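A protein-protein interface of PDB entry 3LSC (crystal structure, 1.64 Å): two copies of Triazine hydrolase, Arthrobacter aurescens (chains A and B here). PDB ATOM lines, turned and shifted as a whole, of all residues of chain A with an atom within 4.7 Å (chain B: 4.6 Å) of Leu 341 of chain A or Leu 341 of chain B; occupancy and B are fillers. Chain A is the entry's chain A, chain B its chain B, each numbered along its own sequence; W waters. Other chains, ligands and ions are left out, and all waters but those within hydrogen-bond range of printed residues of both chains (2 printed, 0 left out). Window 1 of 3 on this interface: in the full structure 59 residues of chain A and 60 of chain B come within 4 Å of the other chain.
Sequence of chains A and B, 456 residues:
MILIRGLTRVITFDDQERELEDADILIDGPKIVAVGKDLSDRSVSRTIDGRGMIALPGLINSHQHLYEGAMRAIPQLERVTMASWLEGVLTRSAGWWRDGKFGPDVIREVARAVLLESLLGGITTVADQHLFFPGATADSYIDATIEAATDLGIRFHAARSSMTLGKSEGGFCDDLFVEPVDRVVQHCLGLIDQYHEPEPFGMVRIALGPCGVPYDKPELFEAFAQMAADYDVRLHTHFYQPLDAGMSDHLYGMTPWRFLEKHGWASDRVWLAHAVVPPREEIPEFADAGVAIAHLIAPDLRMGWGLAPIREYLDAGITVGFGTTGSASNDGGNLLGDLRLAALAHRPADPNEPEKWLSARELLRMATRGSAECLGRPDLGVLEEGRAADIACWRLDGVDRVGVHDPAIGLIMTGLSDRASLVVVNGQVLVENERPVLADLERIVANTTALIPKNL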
ATOM      1  N   ILE A 297     -20.614   9.645  30.316  1.00  0.00           N
ATOM      2  CA  ILE A 297     -20.135  10.820  29.595  1.00  0.00           C
ATOM      3  C   ILE A 297     -20.773  12.134  30.072  1.00  0.00           C
ATOM      4  O   ILE A 297     -20.081  13.147  30.206  1.00  0.00           O
ATOM      5  CB  ILE A 297     -20.312  10.652  28.062  1.00  0.00           C
ATOM      6  CG1 ILE A 297     -19.600  11.777  27.310  1.00  0.00           C
ATOM      7  CG2 ILE A 297     -21.799  10.602  27.673  1.00  0.00           C
ATOM      8  CD1 ILE A 297     -18.086  11.711  27.376  1.00  0.00           C
ATOM      9  N   ALA A 298     -22.079  12.126  30.344  1.00  0.00           N
ATOM     10  CA  ALA A 298     -22.764  13.386  30.653  1.00  0.00           C
ATOM     11  C   ALA A 298     -22.259  14.087  31.937  1.00  0.00           C
ATOM     12  O   ALA A 298     -21.905  15.266  31.897  1.00  0.00           O
ATOM     13  CB  ALA A 298     -24.307  13.200  30.658  1.00  0.00           C
ATOM     14  N   GLY A 337     -29.673   9.339  24.344  1.00  0.00           N
ATOM     15  CA  GLY A 337     -29.203  10.678  24.037  1.00  0.00           C
ATOM     16  C   GLY A 337     -27.756  10.910  24.466  1.00  0.00           C
ATOM     17  O   GLY A 337     -26.975  11.543  23.755  1.00  0.00           O
ATOM     18  N   ASP A 338     -27.403  10.398  25.636  1.00  0.00           N
ATOM     19  CA  ASP A 338     -26.047  10.554  26.135  1.00  0.00           C
ATOM     20  C   ASP A 338     -25.035   9.840  25.237  1.00  0.00           C
ATOM     21  O   ASP A 338     -23.878  10.250  25.151  1.00  0.00           O
ATOM     22  CB  ASP A 338     -25.934  10.063  27.582  1.00  0.00           C
ATOM     23  CG  ASP A 338     -26.613  10.999  28.572  1.00  0.00           C
ATOM     24  OD1 ASP A 338     -27.114  12.070  28.147  1.00  0.00           O
ATOM     25  OD2 ASP A 338     -26.628  10.664  29.779  1.00  0.00           O
ATOM     26  N   LEU A 339     -25.456   8.773  24.567  1.00  0.00           N
ATOM     27  CA  LEU A 339     -24.540   8.100  23.639  1.00  0.00           C
ATOM     28  C   LEU A 339     -24.024   9.030  22.534  1.00  0.00           C
ATOM     29  O   LEU A 339     -22.855   8.947  22.139  1.00  0.00           O
ATOM     30  CB  LEU A 339     -25.184   6.856  23.020  1.00  0.00           C
ATOM     31  CG  LEU A 339     -25.640   5.766  23.992  1.00  0.00           C
ATOM     32  CD1 LEU A 339     -26.221   4.583  23.241  1.00  0.00           C
ATOM     33  CD2 LEU A 339     -24.478   5.304  24.898  1.00  0.00           C
ATOM     34  N   ARG A 340     -24.893   9.895  22.018  1.00  0.00           N
ATOM     35  CA  ARG A 340     -24.470  10.889  21.029  1.00  0.00           C
ATOM     36  C   ARG A 340     -23.402  11.818  21.608  1.00  0.00           C
ATOM     37  O   ARG A 340     -22.437  12.181  20.934  1.00  0.00           O
ATOM     38  CB  ARG A 340     -25.669  11.697  20.510  1.00  0.00           C
ATOM     39  CG  ARG A 340     -25.298  12.770  19.485  1.00  0.00           C
ATOM     40  CD  ARG A 340     -26.533  13.511  18.973  1.00  0.00           C
ATOM     41  NE  ARG A 340     -26.211  14.802  18.362  1.00  0.00           N
ATOM     42  CZ  ARG A 340     -25.702  14.954  17.143  1.00  0.00           C
ATOM     43  NH1 ARG A 340     -25.455  16.175  16.671  1.00  0.00           N
ATOM     44  NH2 ARG A 340     -25.429  13.883  16.395  1.00  0.00           N
ATOM     45  N   LEU A 341     -23.559  12.192  22.872  1.00  0.00           N
ATOM     46  CA  LEU A 341     -22.565  13.030  23.521  1.00  0.00           C
ATOM     47  C   LEU A 341     -21.211  12.351  23.494  1.00  0.00           C
ATOM     48  O   LEU A 341     -20.206  12.993  23.225  1.00  0.00           O
ATOM     49  CB  LEU A 341     -22.930  13.302  24.981  1.00  0.00           C
ATOM     50  CG  LEU A 341     -24.281  13.951  25.247  1.00  0.00           C
ATOM     51  CD1 LEU A 341     -24.536  14.030  26.754  1.00  0.00           C
ATOM     52  CD2 LEU A 341     -24.334  15.332  24.617  1.00  0.00           C
ATOM     53  N   ALA A 342     -21.185  11.063  23.824  1.00  0.00           N
ATOM     54  CA  ALA A 342     -19.927  10.330  23.847  1.00  0.00           C
ATOM     55  C   ALA A 342     -19.378  10.202  22.426  1.00  0.00           C
ATOM     56  O   ALA A 342     -18.186  10.411  22.201  1.00  0.00           O
ATOM     57  CB  ALA A 342     -20.103   8.965  24.496  1.00  0.00           C
ATOM     58  N   ALA A 343     -20.251   9.862  21.481  1.00  0.00           N
ATOM     59  CA  ALA A 343     -19.837   9.689  20.080  1.00  0.00           C
ATOM     60  C   ALA A 343     -19.077  10.895  19.562  1.00  0.00           C
ATOM     61  O   ALA A 343     -18.088  10.760  18.849  1.00  0.00           O
ATOM     62  CB  ALA A 343     -21.054   9.417  19.194  1.00  0.00           C
ATOM     63  N   LEU A 344     -19.541  12.086  19.914  1.00  0.00           N
ATOM     64  CA  LEU A 344     -18.930  13.299  19.389  1.00  0.00           C
ATOM     65  C   LEU A 344     -17.825  13.845  20.300  1.00  0.00           C
ATOM     66  O   LEU A 344     -16.793  14.305  19.823  1.00  0.00           O
ATOM     67  CB  LEU A 344     -20.008  14.355  19.146  1.00  0.00           C
ATOM     68  CG  LEU A 344     -21.032  13.952  18.084  1.00  0.00           C
ATOM     69  CD1 LEU A 344     -22.144  14.972  18.017  1.00  0.00           C
ATOM     70  CD2 LEU A 344     -20.357  13.814  16.719  1.00  0.00           C
ATOM     71  N   ALA A 345     -18.024  13.782  21.613  1.00  0.00           N
ATOM     72  CA  ALA A 345     -17.114  14.475  22.524  1.00  0.00           C
ATOM     73  C   ALA A 345     -15.739  13.828  22.604  1.00  0.00           C
ATOM     74  O   ALA A 345     -14.757  14.499  22.940  1.00  0.00           O
ATOM     75  CB  ALA A 345     -17.726  14.593  23.933  1.00  0.00           C
ATOM     76  N   HIS A 346     -15.667  12.527  22.330  1.00  0.00           N
ATOM     77  CA  HIS A 346     -14.376  11.835  22.387  1.00  0.00           C
ATOM     78  C   HIS A 346     -13.453  12.205  21.218  1.00  0.00           C
ATOM     79  O   HIS A 346     -12.236  12.033  21.300  1.00  0.00           O
ATOM     80  CB  HIS A 346     -14.569  10.316  22.433  1.00  0.00           C
ATOM     81  CG  HIS A 346     -14.850   9.780  23.806  1.00  0.00           C
ATOM     82  ND1 HIS A 346     -13.852   9.485  24.708  1.00  0.00           N
ATOM     83  CD2 HIS A 346     -16.017   9.479  24.425  1.00  0.00           C
ATOM     84  CE1 HIS A 346     -14.388   9.028  25.825  1.00  0.00           C
ATOM     85  NE2 HIS A 346     -15.702   9.023  25.685  1.00  0.00           N
ATOM     86  N   ILE B 297     -21.300  23.654  17.112  1.00  0.00           N
ATOM     87  CA  ILE B 297     -20.654  22.675  17.993  1.00  0.00           C
ATOM     88  C   ILE B 297     -20.617  21.266  17.406  1.00  0.00           C
ATOM     89  O   ILE B 297     -19.607  20.584  17.494  1.00  0.00           O
ATOM     90  CB  ILE B 297     -21.308  22.645  19.404  1.00  0.00           C
ATOM     91  CG1 ILE B 297     -20.484  21.790  20.382  1.00  0.00           C
ATOM     92  CG2 ILE B 297     -22.748  22.143  19.336  1.00  0.00           C
ATOM     93  CD1 ILE B 297     -19.075  22.318  20.618  1.00  0.00           C
ATOM     94  N   ALA B 298     -21.717  20.824  16.803  1.00  0.00           N
ATOM     95  CA  ALA B 298     -21.790  19.446  16.329  1.00  0.00           C
ATOM     96  C   ALA B 298     -20.732  19.075  15.281  1.00  0.00           C
ATOM     97  O   ALA B 298     -20.005  18.103  15.461  1.00  0.00           O
ATOM     98  CB  ALA B 298     -23.204  19.100  15.856  1.00  0.00           C
ATOM     99  N   LEU B 301     -17.112  19.110  16.735  1.00  0.00           N
ATOM    100  CA  LEU B 301     -16.790  17.888  17.469  1.00  0.00           C
ATOM    101  C   LEU B 301     -16.676  16.672  16.559  1.00  0.00           C
ATOM    102  O   LEU B 301     -15.773  15.846  16.721  1.00  0.00           O
ATOM    103  CB  LEU B 301     -17.843  17.608  18.542  1.00  0.00           C
ATOM    104  CG  LEU B 301     -17.937  18.655  19.646  1.00  0.00           C
ATOM    105  CD1 LEU B 301     -18.900  18.176  20.706  1.00  0.00           C
ATOM    106  CD2 LEU B 301     -16.565  18.917  20.250  1.00  0.00           C
ATOM    107  N   GLY B 337     -31.145  20.271  20.274  1.00  0.00           N
ATOM    108  CA  GLY B 337     -30.322  19.176  20.758  1.00  0.00           C
ATOM    109  C   GLY B 337     -28.842  19.529  20.783  1.00  0.00           C
ATOM    110  O   GLY B 337     -28.100  19.142  21.692  1.00  0.00           O
ATOM    111  N   ASP B 338     -28.394  20.275  19.780  1.00  0.00           N
ATOM    112  CA  ASP B 338     -26.979  20.620  19.703  1.00  0.00           C
ATOM    113  C   ASP B 338     -26.576  21.598  20.809  1.00  0.00           C
ATOM    114  O   ASP B 338     -25.406  21.668  21.187  1.00  0.00           O
ATOM    115  CB  ASP B 338     -26.624  21.200  18.329  1.00  0.00           C
ATOM    116  CG  ASP B 338     -26.544  20.141  17.231  1.00  0.00           C
ATOM    117  OD1 ASP B 338     -26.733  18.939  17.517  1.00  0.00           O
ATOM    118  OD2 ASP B 338     -26.288  20.529  16.063  1.00  0.00           O
ATOM    119  N   LEU B 339     -27.541  22.348  21.332  1.00  0.00           N
ATOM    120  CA  LEU B 339     -27.253  23.305  22.396  1.00  0.00           C
ATOM    121  C   LEU B 339     -26.756  22.577  23.632  1.00  0.00           C
ATOM    122  O   LEU B 339     -25.879  23.076  24.341  1.00  0.00           O
ATOM    123  CB  LEU B 339     -28.487  24.133  22.754  1.00  0.00           C
ATOM    124  CG  LEU B 339     -28.974  25.067  21.636  1.00  0.00           C
ATOM    125  CD1 LEU B 339     -30.100  25.955  22.166  1.00  0.00           C
ATOM    126  CD2 LEU B 339     -27.820  25.908  21.079  1.00  0.00           C
ATOM    127  N   ARG B 340     -27.330  21.405  23.891  1.00  0.00           N
ATOM    128  CA  ARG B 340     -26.926  20.597  25.038  1.00  0.00           C
ATOM    129  C   ARG B 340     -25.497  20.110  24.832  1.00  0.00           C
ATOM    130  O   ARG B 340     -24.703  20.084  25.759  1.00  0.00           O
ATOM    131  CB  ARG B 340     -27.867  19.404  25.216  1.00  0.00           C
ATOM    132  CG  ARG B 340     -27.363  18.363  26.217  1.00  0.00           C
ATOM    133  CD  ARG B 340     -28.460  17.362  26.543  1.00  0.00           C
ATOM    134  NE  ARG B 340     -27.969  16.194  27.274  1.00  0.00           N
ATOM    135  CZ  ARG B 340     -27.701  16.184  28.576  1.00  0.00           C
ATOM    136  NH1 ARG B 340     -27.272  15.065  29.151  1.00  0.00           N
ATOM    137  NH2 ARG B 340     -27.844  17.295  29.302  1.00  0.00           N
ATOM    138  N   LEU B 341     -25.175  19.722  23.605  1.00  0.00           N
ATOM    139  CA  LEU B 341     -23.813  19.336  23.279  1.00  0.00           C
ATOM    140  C   LEU B 341     -22.842  20.463  23.646  1.00  0.00           C
ATOM    141  O   LEU B 341     -21.825  20.220  24.288  1.00  0.00           O
ATOM    142  CB  LEU B 341     -23.703  18.985  21.794  1.00  0.00           C
ATOM    143  CG  LEU B 341     -22.380  18.406  21.302  1.00  0.00           C
ATOM    144  CD1 LEU B 341     -21.976  17.167  22.099  1.00  0.00           C
ATOM    145  CD2 LEU B 341     -22.511  18.086  19.815  1.00  0.00           C
ATOM    146  N   ALA B 342     -23.158  21.690  23.242  1.00  0.00           N
ATOM    147  CA  ALA B 342     -22.309  22.833  23.555  1.00  0.00           C
ATOM    148  C   ALA B 342     -22.230  23.066  25.062  1.00  0.00           C
ATOM    149  O   ALA B 342     -21.152  23.301  25.601  1.00  0.00           O
ATOM    150  CB  ALA B 342     -22.811  24.091  22.843  1.00  0.00           C
ATOM    151  N   ALA B 343     -23.377  22.991  25.732  1.00  0.00           N
ATOM    152  CA  ALA B 343     -23.453  23.253  27.172  1.00  0.00           C
ATOM    153  C   ALA B 343     -22.472  22.391  27.946  1.00  0.00           C
ATOM    154  O   ALA B 343     -21.845  22.850  28.906  1.00  0.00           O
ATOM    155  CB  ALA B 343     -24.868  23.019  27.675  1.00  0.00           C
ATOM    156  N   LEU B 344     -22.359  21.133  27.536  1.00  0.00           N
ATOM    157  CA  LEU B 344     -21.532  20.165  28.252  1.00  0.00           C
ATOM    158  C   LEU B 344     -20.095  20.127  27.740  1.00  0.00           C
ATOM    159  O   LEU B 344     -19.143  20.149  28.534  1.00  0.00           O
ATOM    160  CB  LEU B 344     -22.166  18.767  28.196  1.00  0.00           C
ATOM    161  CG  LEU B 344     -23.450  18.578  29.015  1.00  0.00           C
ATOM    162  CD1 LEU B 344     -24.473  19.678  28.745  1.00  0.00           C
ATOM    163  CD2 LEU B 344     -24.077  17.205  28.792  1.00  0.00           C
ATOM    164  N   ALA B 345     -19.934  20.086  26.419  1.00  0.00           N
ATOM    165  CA  ALA B 345     -18.615  19.892  25.821  1.00  0.00           C
ATOM    166  C   ALA B 345     -17.634  21.039  26.076  1.00  0.00           C
ATOM    167  O   ALA B 345     -16.427  20.823  26.085  1.00  0.00           O
ATOM    168  CB  ALA B 345     -18.741  19.612  24.318  1.00  0.00           C
HETATM  169  O   HOH W   1     -27.359  17.027  19.367  1.00  0.00           O
HETATM  170  O   HOH W   2     -27.835  13.685  26.057  1.00  0.00           O
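The side-chain carboxylate (OD1) of Asp 338 of chain A lies within salt-bridge range of the guanidinium group (NH1) of Arg 340 of chain B.
NH1 of Arg 340 of chain A is in salt-bridge range of OD1 of Asp 338 of chain B.
Ala 298 of chain A touches Arg 340 of chain B (CB to NH1, 3.8 Å).
Ala 298 of chain B touches Arg 340 of chain A (CB to NH1, 3.8 Å).
NH1 of Arg 340 of chain B touches CD1 of Leu 341 of chain A (3.8 Å).
CD2 of Leu 341 of chain A touches CD1 of Leu 341 of chain B (3.9 Å).
Leu 341 of chain A touches Leu 344 of chain B (CD1 to CD2, 3.8 Å).
O of Leu 344 of chain A touches O of Leu 301 of chain B, 3.6 Å away.
Leu 341 of chain B touches Leu 344 of chain A (CD2 to CD1, 3.6 Å).
Of the printed residues of chain B, Asp 338 of chain A touches Arg 340 (3.2 Å).
Leu 341 of chain A touches three residues of chain B.
Of the printed residues of chain A, Asp 338 of chain B touches Arg 340.
Of chain A, only Leu 341 and Leu 344 come within 4 Å of Leu 341 of chain B.
The nearest printed residue of chain A that does not touch Leu 341 of chain B is Arg 340 of chain A (4.7 Å).
The nearest printed residue of chain A that does not touch Asp 338 of chain B is Leu 344 of chain A (6.1 Å).
Printed residues of chain A that touch a printed residue of chain B: Ala 298, Asp 338, Arg 340, Leu 341 and Leu 344.
Hydrophobic or aromatic side chains of chain A within 4 Å of the printed part of chain B: Ala 298, Leu 341 and Leu 344.
Printed residues of chain B that touch a printed residue of chain A: Ala 298, Leu 301, Asp 338, Arg 340, Leu 341 and Leu 344.
Hydrophobic or aromatic side chains of chain B that line the printed part of chain A: Ala 298, Leu 301, Leu 341 and Leu 344.
Among the printed residues, 9 pairs touch across the chains.
Among the printed residues, Asp or Glu carboxylates within 4 Å of a Lys or Arg side-chain nitrogen of the other chain: Asp 338 of chain A with Arg 340 of chain B and Arg 340 of chain A with Asp 338 of chain B.
Ala 298 of chain A touches Arg 340 of chain B, and with the chains exchanged Arg 340 of chain A touches Ala 298 of chain B.
Asp 338 of chain A touches Arg 340 of chain B, and with the chains exchanged Arg 340 of chain A touches Asp 338 of chain B.
Leu 341 of chain A touches Arg 340 of chain B, but with the chains exchanged Arg 340 of chain A does not touch Leu 341 of chain B (4.7 Å).
Leu 341 of chain B touches its own counterpart, Leu 341 of chain A.
Positions printed for both chains: 297, 298, 337, 338, 339, 340, 341, 342, 343, 344 and 345.
Water W1 lies within hydrogen-bond range of NE of Arg 340 of chain A (2.7 Å), OD1 of Asp 338 of chain B (2.7 Å) and O of Gly 337 of chain B (3.2 Å).
Water W2 lies within hydrogen-bond range of the side-chain carboxylate of Asp 338 of chain A, the guanidinium group of Arg 340 of chain B and the backbone carbonyl oxygen of Gly 337 of chain A.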
